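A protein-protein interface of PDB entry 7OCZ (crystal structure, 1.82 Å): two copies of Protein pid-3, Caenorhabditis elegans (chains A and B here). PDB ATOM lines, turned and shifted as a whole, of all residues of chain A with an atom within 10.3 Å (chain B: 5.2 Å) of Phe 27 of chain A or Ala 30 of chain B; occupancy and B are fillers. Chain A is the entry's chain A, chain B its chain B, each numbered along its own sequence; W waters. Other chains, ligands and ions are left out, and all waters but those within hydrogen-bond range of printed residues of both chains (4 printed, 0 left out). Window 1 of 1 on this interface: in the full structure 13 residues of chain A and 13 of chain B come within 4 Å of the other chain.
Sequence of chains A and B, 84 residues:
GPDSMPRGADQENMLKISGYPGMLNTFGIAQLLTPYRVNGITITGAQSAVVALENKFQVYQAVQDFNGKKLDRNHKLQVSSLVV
Phe 27 of chain A touches Val 38 of chain B, and with the chains exchanged Val 38 of chain A touches Phe 27 of chain B.
Phe 27 of chain A touches Ile 41 of chain B, and with the chains exchanged Ile 41 of chain A touches Phe 27 of chain B.
Thr 34 of chain A touches its own counterpart, Thr 34 of chain B.
Positions printed for both chains: 4, 26, 27, 28, 29, 30, 31, 32, 33, 34, 38, 39, 40 and 41.
Of the 20 pairs that touch across the chains among the printed residues, 17 have their exchanged pair printed and touching as well.
Among the printed residues, merely in contact across the chains: Asn 25 of chain A with Asn 39 of chain B, Phe 27 of chain A with Ala 30 of chain B, Phe 27 of chain A with Val 38 of chain B, Phe 27 of chain A with Gly 40 of chain B, Phe 27 of chain A with Ile 41 of chain B, Ala 30 of chain A with Phe 27 of chain B, Gln 31 of chain A with Leu 33 of chain B, Gln 31 of chain A with Thr 34 of chain B, Gln 31 of chain A with Val 38 of chain B, Leu 33 of chain A with Gln 31 of chain B, Thr 34 of chain A with Gln 31 of chain B, Thr 34 of chain A with Thr 34 of chain B, Val 38 of chain A with Phe 27 of chain B, Val 38 of chain A with Gln 31 of chain B, Gly 40 of chain A with Phe 27 of chain B and Ile 41 of chain A with Phe 27 of chain B.
Water W2 bridges the side-chain amide oxygen of Asn 39 of chain B (2.8 Å) and the side-chain amide nitrogen of Asn 25 of chain A (3.0 Å).
Water W1 lies within hydrogen-bond range of OE1 of Gln 31 of chain A (2.9 Å), N of Val 38 of chain B (2.9 Å), OD1 of Asn 25 of chain A (3.1 Å) and N of Gly 28 of chain A (3.3 Å).
Water W4 lies within hydrogen-bond range of OE1 of Gln 31 of chain B (2.9 Å) and O of Pro 35 of chain A (3.3 Å).
The side-chain hydroxyl (OG1) of Thr 34 of chain A lies within hydrogen-bond range of the backbone carbonyl oxygen (O) of Gln 31 of chain A.
O of Ser 4 of chain B is in hydrogen-bond range of N of Ile 41 of chain B (3.0 Å).
O of Gln 31 of chain B lies within hydrogen-bond range of OG1 of Thr 34 of chain B, at 2.6 Å.
The side-chain amide oxygen of Asn 25 of chain A sits at hydrogen-bond distance from the backbone NH of Gly 28 of chain A (2.8 Å).
O of Ser 4 of chain A lies within hydrogen-bond range of N of Ile 41 of chain A, 2.7 Å away.
The backbone carbonyl oxygen of Ala 30 of chain A is in hydrogen-bond range of the side-chain amide nitrogen of Gln 31 of chain B, 2.9 Å away.
The side-chain amide nitrogen (ND2) of Asn 25 of chain A sits at hydrogen-bond distance from the backbone carbonyl oxygen (O) of Val 38 of chain B.
O of Tyr 36 of chain A is in hydrogen-bond range of NE2 of Gln 31 of chain B (2.9 Å).
O of Ala 30 of chain B is in hydrogen-bond range of NE2 of Gln 31 of chain A.
Printed residues of chain A that touch a printed residue of chain B: Asn 25, Phe 27, Ala 30, Gln 31, Leu 33, Thr 34, Tyr 36, Val 38, Gly 40 and Ile 41.
Hydrophobic or aromatic side chains of chain B within 4 Å of the printed part of chain A: Phe 27, Ala 30, Val 38 and Ile 41.
Among the printed residues, no Asp or Glu carboxylate lies within 4 Å of a Lys or Arg side-chain nitrogen of the other chain.
Printed residues of chain B within 4 Å of Asn 25 of chain A: Val 38 and Asn 39.
Printed residues of chain B within 4 Å of Phe 27 of chain A: Ala 30, Val 38, Gly 40 and Ile 41.
Pro 35 of chain A touches none of the printed residues of chain B.
Of the printed residues of chain B, Gly 40 of chain A touches Phe 27 (3.7 Å).
No residue of chain A comes within 4 Å of Gly 28 of chain B.
Printed residues of chain A within 4 Å of Ala 30 of chain B: Phe 27 and Gln 31.
Of the printed residues of chain A, Gln 31 of chain B touches Ala 30, Leu 33, Thr 34, Tyr 36 and Val 38.
Of chain A, only Gln 31 and Thr 34 come within 4 Å of Thr 34 of chain B.
Val 38 of chain B touches three residues of chain A.
Of chain A, only Phe 27 (3.7 Å) comes within 4 Å of Gly 40 of chain B.
Ile 41 of chain B touches just one residue of chain A: Phe 27 (3.8 Å).
The nearest residue of chain A that does not touch Ala 30 of chain B is Ala 30 of chain A (5.4 Å).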
ATOM      1  N   SER A   4      33.835   8.894   1.091  1.00  0.00           N
ATOM      2  CA  SER A   4      32.764   7.949   0.797  1.00  0.00           C
ATOM      3  C   SER A   4      32.766   6.767   1.770  1.00  0.00           C
ATOM      4  O   SER A   4      32.018   6.764   2.745  1.00  0.00           O
ATOM      5  CB  SER A   4      32.876   7.442  -0.646  1.00  0.00           C
ATOM      6  N   TYR A  20      14.761   6.020  -0.928  1.00  0.00           N
ATOM      7  CA  TYR A  20      14.699   7.356  -0.360  1.00  0.00           C
ATOM      8  C   TYR A  20      14.614   8.404  -1.475  1.00  0.00           C
ATOM      9  O   TYR A  20      14.919   8.114  -2.635  1.00  0.00           O
ATOM     10  CB  TYR A  20      15.923   7.602   0.523  1.00  0.00           C
ATOM     11  CG  TYR A  20      17.224   7.280  -0.157  1.00  0.00           C
ATOM     12  CD1 TYR A  20      17.838   8.201  -1.000  1.00  0.00           C
ATOM     13  CD2 TYR A  20      17.831   6.048   0.026  1.00  0.00           C
ATOM     14  CE1 TYR A  20      19.022   7.906  -1.632  1.00  0.00           C
ATOM     15  CE2 TYR A  20      19.015   5.745  -0.596  1.00  0.00           C
ATOM     16  CZ  TYR A  20      19.604   6.675  -1.429  1.00  0.00           C
ATOM     17  OH  TYR A  20      20.788   6.370  -2.052  1.00  0.00           O
ATOM     18  N   PRO A  21      14.201   9.633  -1.152  1.00  0.00           N
ATOM     19  CA  PRO A  21      14.142  10.674  -2.188  1.00  0.00           C
ATOM     20  C   PRO A  21      15.526  10.978  -2.739  1.00  0.00           C
ATOM     21  O   PRO A  21      16.492  11.140  -1.989  1.00  0.00           O
ATOM     22  CB  PRO A  21      13.543  11.880  -1.456  1.00  0.00           C
ATOM     23  CG  PRO A  21      12.833  11.305  -0.281  1.00  0.00           C
ATOM     24  CD  PRO A  21      13.620  10.093   0.122  1.00  0.00           C
ATOM     25  N   MET A  23      16.823  13.510  -3.752  1.00  0.00           N
ATOM     26  CA  MET A  23      17.397  14.777  -3.320  1.00  0.00           C
ATOM     27  C   MET A  23      18.484  14.610  -2.255  1.00  0.00           C
ATOM     28  O   MET A  23      19.324  15.506  -2.110  1.00  0.00           O
ATOM     29  CB  MET A  23      16.272  15.670  -2.802  1.00  0.00           C
ATOM     30  CG  MET A  23      16.097  15.597  -1.303  1.00  0.00           C
ATOM     31  SD  MET A  23      15.194  17.011  -0.668  1.00  0.00           S
ATOM     32  CE  MET A  23      13.827  17.026  -1.821  1.00  0.00           C
ATOM     33  N   LEU A  24      18.501  13.493  -1.521  1.00  0.00           N
ATOM     34  CA  LEU A  24      19.429  13.351  -0.404  1.00  0.00           C
ATOM     35  C   LEU A  24      20.869  13.209  -0.884  1.00  0.00           C
ATOM     36  O   LEU A  24      21.151  12.471  -1.831  1.00  0.00           O
ATOM     37  CB  LEU A  24      19.067  12.131   0.444  1.00  0.00           C
ATOM     38  CG  LEU A  24      17.740  12.095   1.180  1.00  0.00           C
ATOM     39  CD1 LEU A  24      17.739  10.919   2.171  1.00  0.00           C
ATOM     40  CD2 LEU A  24      17.507  13.412   1.897  1.00  0.00           C
ATOM     41  N   ASN A  25      21.791  13.900  -0.206  1.00  0.00           N
ATOM     42  CA  ASN A  25      23.210  13.645  -0.414  1.00  0.00           C
ATOM     43  C   ASN A  25      23.672  12.576   0.584  1.00  0.00           C
ATOM     44  O   ASN A  25      22.865  12.022   1.337  1.00  0.00           O
ATOM     45  CB  ASN A  25      24.019  14.946  -0.317  1.00  0.00           C
ATOM     46  CG  ASN A  25      23.868  15.657   1.025  1.00  0.00           C
ATOM     47  OD1 ASN A  25      23.303  15.120   1.977  1.00  0.00           O
ATOM     48  ND2 ASN A  25      24.353  16.898   1.088  1.00  0.00           N
ATOM     49  N   THR A  26      24.975  12.255   0.594  1.00  0.00           N
ATOM     50  CA  THR A  26      25.441  11.191   1.488  1.00  0.00           C
ATOM     51  C   THR A  26      25.225  11.565   2.951  1.00  0.00           C
ATOM     52  O   THR A  26      24.847  10.715   3.765  1.00  0.00           O
ATOM     53  CB  THR A  26      26.912  10.847   1.237  1.00  0.00           C
ATOM     54  OG1 THR A  26      27.740  11.963   1.577  1.00  0.00           O
ATOM     55  CG2 THR A  26      27.139  10.468  -0.215  1.00  0.00           C
ATOM     56  N   PHE A  27      25.430  12.840   3.300  1.00  0.00           N
ATOM     57  CA  PHE A  27      25.145  13.277   4.665  1.00  0.00           C
ATOM     58  C   PHE A  27      23.677  13.077   5.012  1.00  0.00           C
ATOM     59  O   PHE A  27      23.345  12.683   6.137  1.00  0.00           O
ATOM     60  CB  PHE A  27      25.533  14.744   4.855  1.00  0.00           C
ATOM     61  CG  PHE A  27      27.016  14.980   4.934  1.00  0.00           C
ATOM     62  CD1 PHE A  27      27.783  14.328   5.890  1.00  0.00           C
ATOM     63  CD2 PHE A  27      27.638  15.867   4.069  1.00  0.00           C
ATOM     64  CE1 PHE A  27      29.149  14.550   5.974  1.00  0.00           C
ATOM     65  CE2 PHE A  27      29.002  16.091   4.146  1.00  0.00           C
ATOM     66  CZ  PHE A  27      29.757  15.435   5.103  1.00  0.00           C
ATOM     67  N   GLY A  28      22.783  13.362   4.061  1.00  0.00           N
ATOM     68  CA  GLY A  28      21.363  13.166   4.297  1.00  0.00           C
ATOM     69  C   GLY A  28      20.980  11.712   4.467  1.00  0.00           C
ATOM     70  O   GLY A  28      20.048  11.394   5.215  1.00  0.00           O
ATOM     71  N   ILE A  29      21.674  10.809   3.773  1.00  0.00           N
ATOM     72  CA  ILE A  29      21.435   9.384   3.982  1.00  0.00           C
ATOM     73  C   ILE A  29      21.844   8.971   5.390  1.00  0.00           C
ATOM     74  O   ILE A  29      21.145   8.193   6.051  1.00  0.00           O
ATOM     75  CB  ILE A  29      22.168   8.558   2.914  1.00  0.00           C
ATOM     76  CG1 ILE A  29      21.585   8.853   1.540  1.00  0.00           C
ATOM     77  CG2 ILE A  29      22.085   7.066   3.228  1.00  0.00           C
ATOM     78  CD1 ILE A  29      22.476   8.399   0.445  1.00  0.00           C
ATOM     79  N   ALA A  30      22.980   9.476   5.880  1.00  0.00           N
ATOM     80  CA  ALA A  30      23.343   9.198   7.267  1.00  0.00           C
ATOM     81  C   ALA A  30      22.309   9.782   8.222  1.00  0.00           C
ATOM     82  O   ALA A  30      21.954   9.154   9.226  1.00  0.00           O
ATOM     83  CB  ALA A  30      24.735   9.747   7.571  1.00  0.00           C
ATOM     84  N   GLN A  31      21.796  10.977   7.912  1.00  0.00           N
ATOM     85  CA  GLN A  31      20.765  11.578   8.757  1.00  0.00           C
ATOM     86  C   GLN A  31      19.501  10.735   8.779  1.00  0.00           C
ATOM     87  O   GLN A  31      18.814  10.661   9.807  1.00  0.00           O
ATOM     88  CB  GLN A  31      20.450  12.988   8.269  1.00  0.00           C
ATOM     89  CG  GLN A  31      21.557  13.980   8.558  1.00  0.00           C
ATOM     90  CD  GLN A  31      21.314  15.306   7.885  1.00  0.00           C
ATOM     91  OE1 GLN A  31      20.928  15.357   6.718  1.00  0.00           O
ATOM     92  NE2 GLN A  31      21.544  16.395   8.614  1.00  0.00           N
ATOM     93  N   LEU A  32      19.183  10.090   7.657  1.00  0.00           N
ATOM     94  CA  LEU A  32      18.011   9.225   7.577  1.00  0.00           C
ATOM     95  C   LEU A  32      18.103   8.072   8.567  1.00  0.00           C
ATOM     96  O   LEU A  32      17.081   7.615   9.094  1.00  0.00           O
ATOM     97  CB  LEU A  32      17.892   8.695   6.148  1.00  0.00           C
ATOM     98  CG  LEU A  32      16.733   7.803   5.711  1.00  0.00           C
ATOM     99  CD1 LEU A  32      15.429   8.206   6.386  1.00  0.00           C
ATOM    100  CD2 LEU A  32      16.607   7.820   4.199  1.00  0.00           C
ATOM    101  N   LEU A  33      19.321   7.605   8.839  1.00  0.00           N
ATOM    102  CA  LEU A  33      19.599   6.412   9.623  1.00  0.00           C
ATOM    103  C   LEU A  33      19.958   6.716  11.076  1.00  0.00           C
ATOM    104  O   LEU A  33      20.407   5.816  11.790  1.00  0.00           O
ATOM    105  CB  LEU A  33      20.738   5.633   8.962  1.00  0.00           C
ATOM    106  CG  LEU A  33      20.427   5.070   7.574  1.00  0.00           C
ATOM    107  CD1 LEU A  33      21.679   4.502   6.928  1.00  0.00           C
ATOM    108  CD2 LEU A  33      19.364   3.999   7.686  1.00  0.00           C
ATOM    109  N   THR A  34      19.804   7.960  11.514  1.00  0.00           N
ATOM    110  CA  THR A  34      20.049   8.302  12.910  1.00  0.00           C
ATOM    111  C   THR A  34      19.243   7.366  13.807  1.00  0.00           C
ATOM    112  O   THR A  34      18.096   7.044  13.475  1.00  0.00           O
ATOM    113  CB  THR A  34      19.647   9.762  13.162  1.00  0.00           C
ATOM    114  OG1 THR A  34      20.250  10.602  12.172  1.00  0.00           O
ATOM    115  CG2 THR A  34      20.073  10.242  14.525  1.00  0.00           C
ATOM    116  N   PRO A  35      19.797   6.900  14.944  1.00  0.00           N
ATOM    117  CA  PRO A  35      21.100   7.172  15.563  1.00  0.00           C
ATOM    118  C   PRO A  35      22.168   6.125  15.298  1.00  0.00           C
ATOM    119  O   PRO A  35      23.095   5.999  16.110  1.00  0.00           O
ATOM    120  CB  PRO A  35      20.759   7.184  17.047  1.00  0.00           C
ATOM    121  CG  PRO A  35      19.709   6.092  17.157  1.00  0.00           C
ATOM    122  CD  PRO A  35      19.002   6.002  15.804  1.00  0.00           C
ATOM    123  N   TYR A  36      22.048   5.378  14.205  1.00  0.00           N
ATOM    124  CA  TYR A  36      23.035   4.346  13.928  1.00  0.00           C
ATOM    125  C   TYR A  36      24.351   4.985  13.523  1.00  0.00           C
ATOM    126  O   TYR A  36      24.379   5.923  12.723  1.00  0.00           O
ATOM    127  CB  TYR A  36      22.539   3.404  12.830  1.00  0.00           C
ATOM    128  CG  TYR A  36      21.462   2.460  13.304  1.00  0.00           C
ATOM    129  CD1 TYR A  36      21.793   1.237  13.871  1.00  0.00           C
ATOM    130  CD2 TYR A  36      20.118   2.790  13.190  1.00  0.00           C
ATOM    131  CE1 TYR A  36      20.819   0.365  14.313  1.00  0.00           C
ATOM    132  CE2 TYR A  36      19.128   1.921  13.631  1.00  0.00           C
ATOM    133  CZ  TYR A  36      19.492   0.708  14.196  1.00  0.00           C
ATOM    134  OH  TYR A  36      18.518  -0.160  14.646  1.00  0.00           O
ATOM    135  N   VAL A  38      27.365   5.472  11.368  1.00  0.00           N
ATOM    136  CA  VAL A  38      27.630   5.255   9.949  1.00  0.00           C
ATOM    137  C   VAL A  38      29.097   5.569   9.709  1.00  0.00           C
ATOM    138  O   VAL A  38      29.557   6.674  10.021  1.00  0.00           O
ATOM    139  CB  VAL A  38      26.733   6.141   9.070  1.00  0.00           C
ATOM    140  CG1 VAL A  38      27.148   6.037   7.610  1.00  0.00           C
ATOM    141  CG2 VAL A  38      25.269   5.758   9.250  1.00  0.00           C
ATOM    142  N   ASN A  39      29.834   4.606   9.158  1.00  0.00           N
ATOM    143  CA  ASN A  39      31.271   4.743   8.951  1.00  0.00           C
ATOM    144  C   ASN A  39      31.655   5.004   7.505  1.00  0.00           C
ATOM    145  O   ASN A  39      32.802   5.384   7.240  1.00  0.00           O
ATOM    146  CB  ASN A  39      31.989   3.485   9.434  1.00  0.00           C
ATOM    147  CG  ASN A  39      31.901   3.320  10.923  1.00  0.00           C
ATOM    148  OD1 ASN A  39      31.967   4.299  11.667  1.00  0.00           O
ATOM    149  ND2 ASN A  39      31.728   2.083  11.374  1.00  0.00           N
ATOM    150  N   GLY A  40      30.740   4.792   6.572  1.00  0.00           N
ATOM    151  CA  GLY A  40      30.972   5.128   5.186  1.00  0.00           C
ATOM    152  C   GLY A  40      29.703   4.941   4.388  1.00  0.00           C
ATOM    153  O   GLY A  40      28.817   4.185   4.801  1.00  0.00           O
ATOM    154  N   ILE A  41      29.594   5.635   3.258  1.00  0.00           N
ATOM    155  CA  ILE A  41      28.436   5.542   2.375  1.00  0.00           C
ATOM    156  C   ILE A  41      28.935   5.574   0.940  1.00  0.00           C
ATOM    157  O   ILE A  41      29.744   6.436   0.581  1.00  0.00           O
ATOM    158  CB  ILE A  41      27.425   6.684   2.610  1.00  0.00           C
ATOM    159  CG1 ILE A  41      26.831   6.605   4.023  1.00  0.00           C
ATOM    160  CG2 ILE A  41      26.323   6.656   1.551  1.00  0.00           C
ATOM    161  CD1 ILE A  41      25.855   7.717   4.359  1.00  0.00           C
ATOM    162  N   THR A  42      28.457   4.642   0.122  1.00  0.00           N
ATOM    163  CA  THR A  42      28.712   4.641  -1.312  1.00  0.00           C
ATOM    164  C   THR A  42      27.389   4.769  -2.047  1.00  0.00           C
ATOM    165  O   THR A  42      26.511   3.913  -1.892  1.00  0.00           O
ATOM    166  CB  THR A  42      29.423   3.364  -1.748  1.00  0.00           C
ATOM    167  OG1 THR A  42      30.710   3.295  -1.122  1.00  0.00           O
ATOM    168  CG2 THR A  42      29.567   3.341  -3.267  1.00  0.00           C
ATOM    169  N   ILE A  43      27.248   5.827  -2.841  1.00  0.00           N
ATOM    170  CA  ILE A  43      26.055   6.024  -3.659  1.00  0.00           C
ATOM    171  C   ILE A  43      26.136   5.083  -4.853  1.00  0.00           C
ATOM    172  O   ILE A  43      27.113   5.115  -5.609  1.00  0.00           O
ATOM    173  CB  ILE A  43      25.932   7.479  -4.128  1.00  0.00           C
ATOM    174  CG1 ILE A  43      25.918   8.442  -2.950  1.00  0.00           C
ATOM    175  CG2 ILE A  43      24.670   7.649  -4.950  1.00  0.00           C
ATOM    176  CD1 ILE A  43      24.742   8.276  -2.081  1.00  0.00           C
ATOM    177  N   ALA A  49      22.022   3.194  -2.108  1.00  0.00           N
ATOM    178  CA  ALA A  49      23.359   3.327  -1.545  1.00  0.00           C
ATOM    179  C   ALA A  49      23.704   2.067  -0.768  1.00  0.00           C
ATOM    180  O   ALA A  49      22.850   1.222  -0.494  1.00  0.00           O
ATOM    181  CB  ALA A  49      23.472   4.558  -0.635  1.00  0.00           C
ATOM    182  N   VAL A  51      25.812   1.264   2.892  1.00  0.00           N
ATOM    183  CA  VAL A  51      26.183   1.999   4.095  1.00  0.00           C
ATOM    184  C   VAL A  51      26.905   1.056   5.048  1.00  0.00           C
ATOM    185  O   VAL A  51      26.409  -0.036   5.340  1.00  0.00           O
ATOM    186  CB  VAL A  51      24.941   2.614   4.771  1.00  0.00           C
ATOM    187  CG1 VAL A  51      25.317   3.307   6.070  1.00  0.00           C
ATOM    188  CG2 VAL A  51      24.220   3.566   3.820  1.00  0.00           C
ATOM    189  N   SER B   4      34.442  15.734   4.545  1.00  0.00           N
ATOM    190  CA  SER B   4      35.115  16.664   3.644  1.00  0.00           C
ATOM    191  C   SER B   4      34.240  17.885   3.338  1.00  0.00           C
ATOM    192  O   SER B   4      33.036  17.883   3.606  1.00  0.00           O
ATOM    193  CB  SER B   4      35.517  15.957   2.345  1.00  0.00           C
ATOM    194  N   THR B  26      32.414  12.281  11.208  1.00  0.00           N
ATOM    195  CA  THR B  26      31.772  13.330  10.414  1.00  0.00           C
ATOM    196  C   THR B  26      30.307  13.011  10.142  1.00  0.00           C
ATOM    197  O   THR B  26      29.458  13.913  10.138  1.00  0.00           O
ATOM    198  CB  THR B  26      32.510  13.542   9.094  1.00  0.00           C
ATOM    199  OG1 THR B  26      32.662  12.285   8.428  1.00  0.00           O
ATOM    200  CG2 THR B  26      33.874  14.163   9.335  1.00  0.00           C
ATOM    201  N   PHE B  27      29.986  11.736   9.907  1.00  0.00           N
ATOM    202  CA  PHE B  27      28.589  11.375   9.690  1.00  0.00           C
ATOM    203  C   PHE B  27      27.759  11.622  10.940  1.00  0.00           C
ATOM    204  O   PHE B  27      26.606  12.068  10.847  1.00  0.00           O
ATOM    205  CB  PHE B  27      28.480   9.917   9.245  1.00  0.00           C
ATOM    206  CG  PHE B  27      28.956   9.683   7.842  1.00  0.00           C
ATOM    207  CD1 PHE B  27      28.333  10.312   6.777  1.00  0.00           C
ATOM    208  CD2 PHE B  27      30.042   8.866   7.588  1.00  0.00           C
ATOM    209  CE1 PHE B  27      28.774  10.112   5.478  1.00  0.00           C
ATOM    210  CE2 PHE B  27      30.482   8.659   6.292  1.00  0.00           C
ATOM    211  CZ  PHE B  27      29.851   9.284   5.239  1.00  0.00           C
ATOM    212  N   GLY B  28      28.328  11.347  12.120  1.00  0.00           N
ATOM    213  CA  GLY B  28      27.596  11.565  13.355  1.00  0.00           C
ATOM    214  C   GLY B  28      27.336  13.029  13.631  1.00  0.00           C
ATOM    215  O   GLY B  28      26.305  13.383  14.219  1.00  0.00           O
ATOM    216  N   ILE B  29      28.257  13.898  13.214  1.00  0.00           N
ATOM    217  CA  ILE B  29      28.026  15.332  13.344  1.00  0.00           C
ATOM    218  C   ILE B  29      26.866  15.767  12.454  1.00  0.00           C
ATOM    219  O   ILE B  29      26.000  16.544  12.876  1.00  0.00           O
ATOM    220  CB  ILE B  29      29.324  16.099  13.038  1.00  0.00           C
ATOM    221  CG1 ILE B  29      30.387  15.711  14.061  1.00  0.00           C
ATOM    222  CG2 ILE B  29      29.103  17.607  13.099  1.00  0.00           C
ATOM    223  CD1 ILE B  29      31.771  16.073  13.641  1.00  0.00           C
ATOM    224  N   ALA B  30      26.808  15.258  11.221  1.00  0.00           N
ATOM    225  CA  ALA B  30      25.637  15.511  10.386  1.00  0.00           C
ATOM    226  C   ALA B  30      24.371  14.987  11.048  1.00  0.00           C
ATOM    227  O   ALA B  30      23.321  15.635  11.000  1.00  0.00           O
ATOM    228  CB  ALA B  30      25.823  14.873   9.008  1.00  0.00           C
ATOM    229  N   GLN B  31      24.447  13.809  11.668  1.00  0.00           N
ATOM    230  CA  GLN B  31      23.261  13.249  12.307  1.00  0.00           C
ATOM    231  C   GLN B  31      22.797  14.112  13.476  1.00  0.00           C
ATOM    232  O   GLN B  31      21.585  14.252  13.695  1.00  0.00           O
ATOM    233  CB  GLN B  31      23.543  11.818  12.749  1.00  0.00           C
ATOM    234  CG  GLN B  31      23.634  10.823  11.599  1.00  0.00           C
ATOM    235  CD  GLN B  31      24.116   9.462  12.070  1.00  0.00           C
ATOM    236  OE1 GLN B  31      25.050   9.368  12.862  1.00  0.00           O
ATOM    237  NE2 GLN B  31      23.471   8.408  11.600  1.00  0.00           N
ATOM    238  N   LEU B  32      23.739  14.709  14.216  1.00  0.00           N
ATOM    239  CA  LEU B  32      23.398  15.674  15.264  1.00  0.00           C
ATOM    240  C   LEU B  32      22.469  16.761  14.754  1.00  0.00           C
ATOM    241  O   LEU B  32      21.603  17.251  15.491  1.00  0.00           O
ATOM    242  CB  LEU B  32      24.659  16.343  15.801  1.00  0.00           C
ATOM    243  CG  LEU B  32      25.417  15.770  16.972  1.00  0.00           C
ATOM    244  CD1 LEU B  32      26.576  16.701  17.285  1.00  0.00           C
ATOM    245  CD2 LEU B  32      24.470  15.662  18.143  1.00  0.00           C
ATOM    246  N   LEU B  33      22.666  17.180  13.508  1.00  0.00           N
ATOM    247  CA  LEU B  33      22.027  18.355  12.946  1.00  0.00           C
ATOM    248  C   LEU B  33      20.786  18.025  12.127  1.00  0.00           C
ATOM    249  O   LEU B  33      20.259  18.910  11.447  1.00  0.00           O
ATOM    250  CB  LEU B  33      23.036  19.122  12.093  1.00  0.00           C
ATOM    251  CG  LEU B  33      24.224  19.653  12.897  1.00  0.00           C
ATOM    252  CD1 LEU B  33      25.252  20.236  11.967  1.00  0.00           C
ATOM    253  CD2 LEU B  33      23.736  20.716  13.866  1.00  0.00           C
ATOM    254  N   THR B  34      20.310  16.783  12.179  1.00  0.00           N
ATOM    255  CA  THR B  34      19.111  16.419  11.432  1.00  0.00           C
ATOM    256  C   THR B  34      17.974  17.355  11.836  1.00  0.00           C
ATOM    257  O   THR B  34      17.857  17.702  13.016  1.00  0.00           O
ATOM    258  CB  THR B  34      18.727  14.962  11.713  1.00  0.00           C
ATOM    259  OG1 THR B  34      19.897  14.140  11.656  1.00  0.00           O
ATOM    260  CG2 THR B  34      17.747  14.445  10.672  1.00  0.00           C
ATOM    261  N   VAL B  38      23.114  19.270   5.091  1.00  0.00           N
ATOM    262  CA  VAL B  38      24.535  19.519   5.311  1.00  0.00           C
ATOM    263  C   VAL B  38      25.251  19.292   3.986  1.00  0.00           C
ATOM    264  O   VAL B  38      25.128  18.219   3.385  1.00  0.00           O
ATOM    265  CB  VAL B  38      25.110  18.609   6.410  1.00  0.00           C
ATOM    266  CG1 VAL B  38      26.618  18.784   6.515  1.00  0.00           C
ATOM    267  CG2 VAL B  38      24.435  18.871   7.755  1.00  0.00           C
ATOM    268  N   ASN B  39      26.006  20.290   3.526  1.00  0.00           N
ATOM    269  CA  ASN B  39      26.746  20.157   2.274  1.00  0.00           C
ATOM    270  C   ASN B  39      28.223  19.853   2.460  1.00  0.00           C
ATOM    271  O   ASN B  39      28.891  19.505   1.482  1.00  0.00           O
ATOM    272  CB  ASN B  39      26.583  21.421   1.423  1.00  0.00           C
ATOM    273  CG  ASN B  39      25.137  21.653   1.013  1.00  0.00           C
ATOM    274  OD1 ASN B  39      24.455  20.730   0.553  1.00  0.00           O
ATOM    275  ND2 ASN B  39      24.660  22.883   1.178  1.00  0.00           N
ATOM    276  N   GLY B  40      28.747  19.974   3.668  1.00  0.00           N
ATOM    277  CA  GLY B  40      30.128  19.612   3.924  1.00  0.00           C
ATOM    278  C   GLY B  40      30.442  19.827   5.387  1.00  0.00           C
ATOM    279  O   GLY B  40      29.750  20.572   6.088  1.00  0.00           O
ATOM    280  N   ILE B  41      31.497  19.148   5.842  1.00  0.00           N
ATOM    281  CA  ILE B  41      31.926  19.206   7.239  1.00  0.00           C
ATOM    282  C   ILE B  41      33.445  19.136   7.287  1.00  0.00           C
ATOM    283  O   ILE B  41      34.054  18.266   6.655  1.00  0.00           O
ATOM    284  CB  ILE B  41      31.315  18.065   8.082  1.00  0.00           C
ATOM    285  CG1 ILE B  41      29.783  18.181   8.130  1.00  0.00           C
ATOM    286  CG2 ILE B  41      31.911  18.064   9.509  1.00  0.00           C
ATOM    287  CD1 ILE B  41      29.091  17.023   8.818  1.00  0.00           C
HETATM  288  O   HOH W   1      22.087  16.612   4.427  1.00  0.00           O
HETATM  289  O   HOH W   2      25.274  18.624  -1.149  1.00  0.00           O
HETATM  290  O   HOH W   3      27.712   8.298  12.587  1.00  0.00           O
HETATM  291  O   HOH W   4      25.519   8.199  15.458  1.00  0.00           O
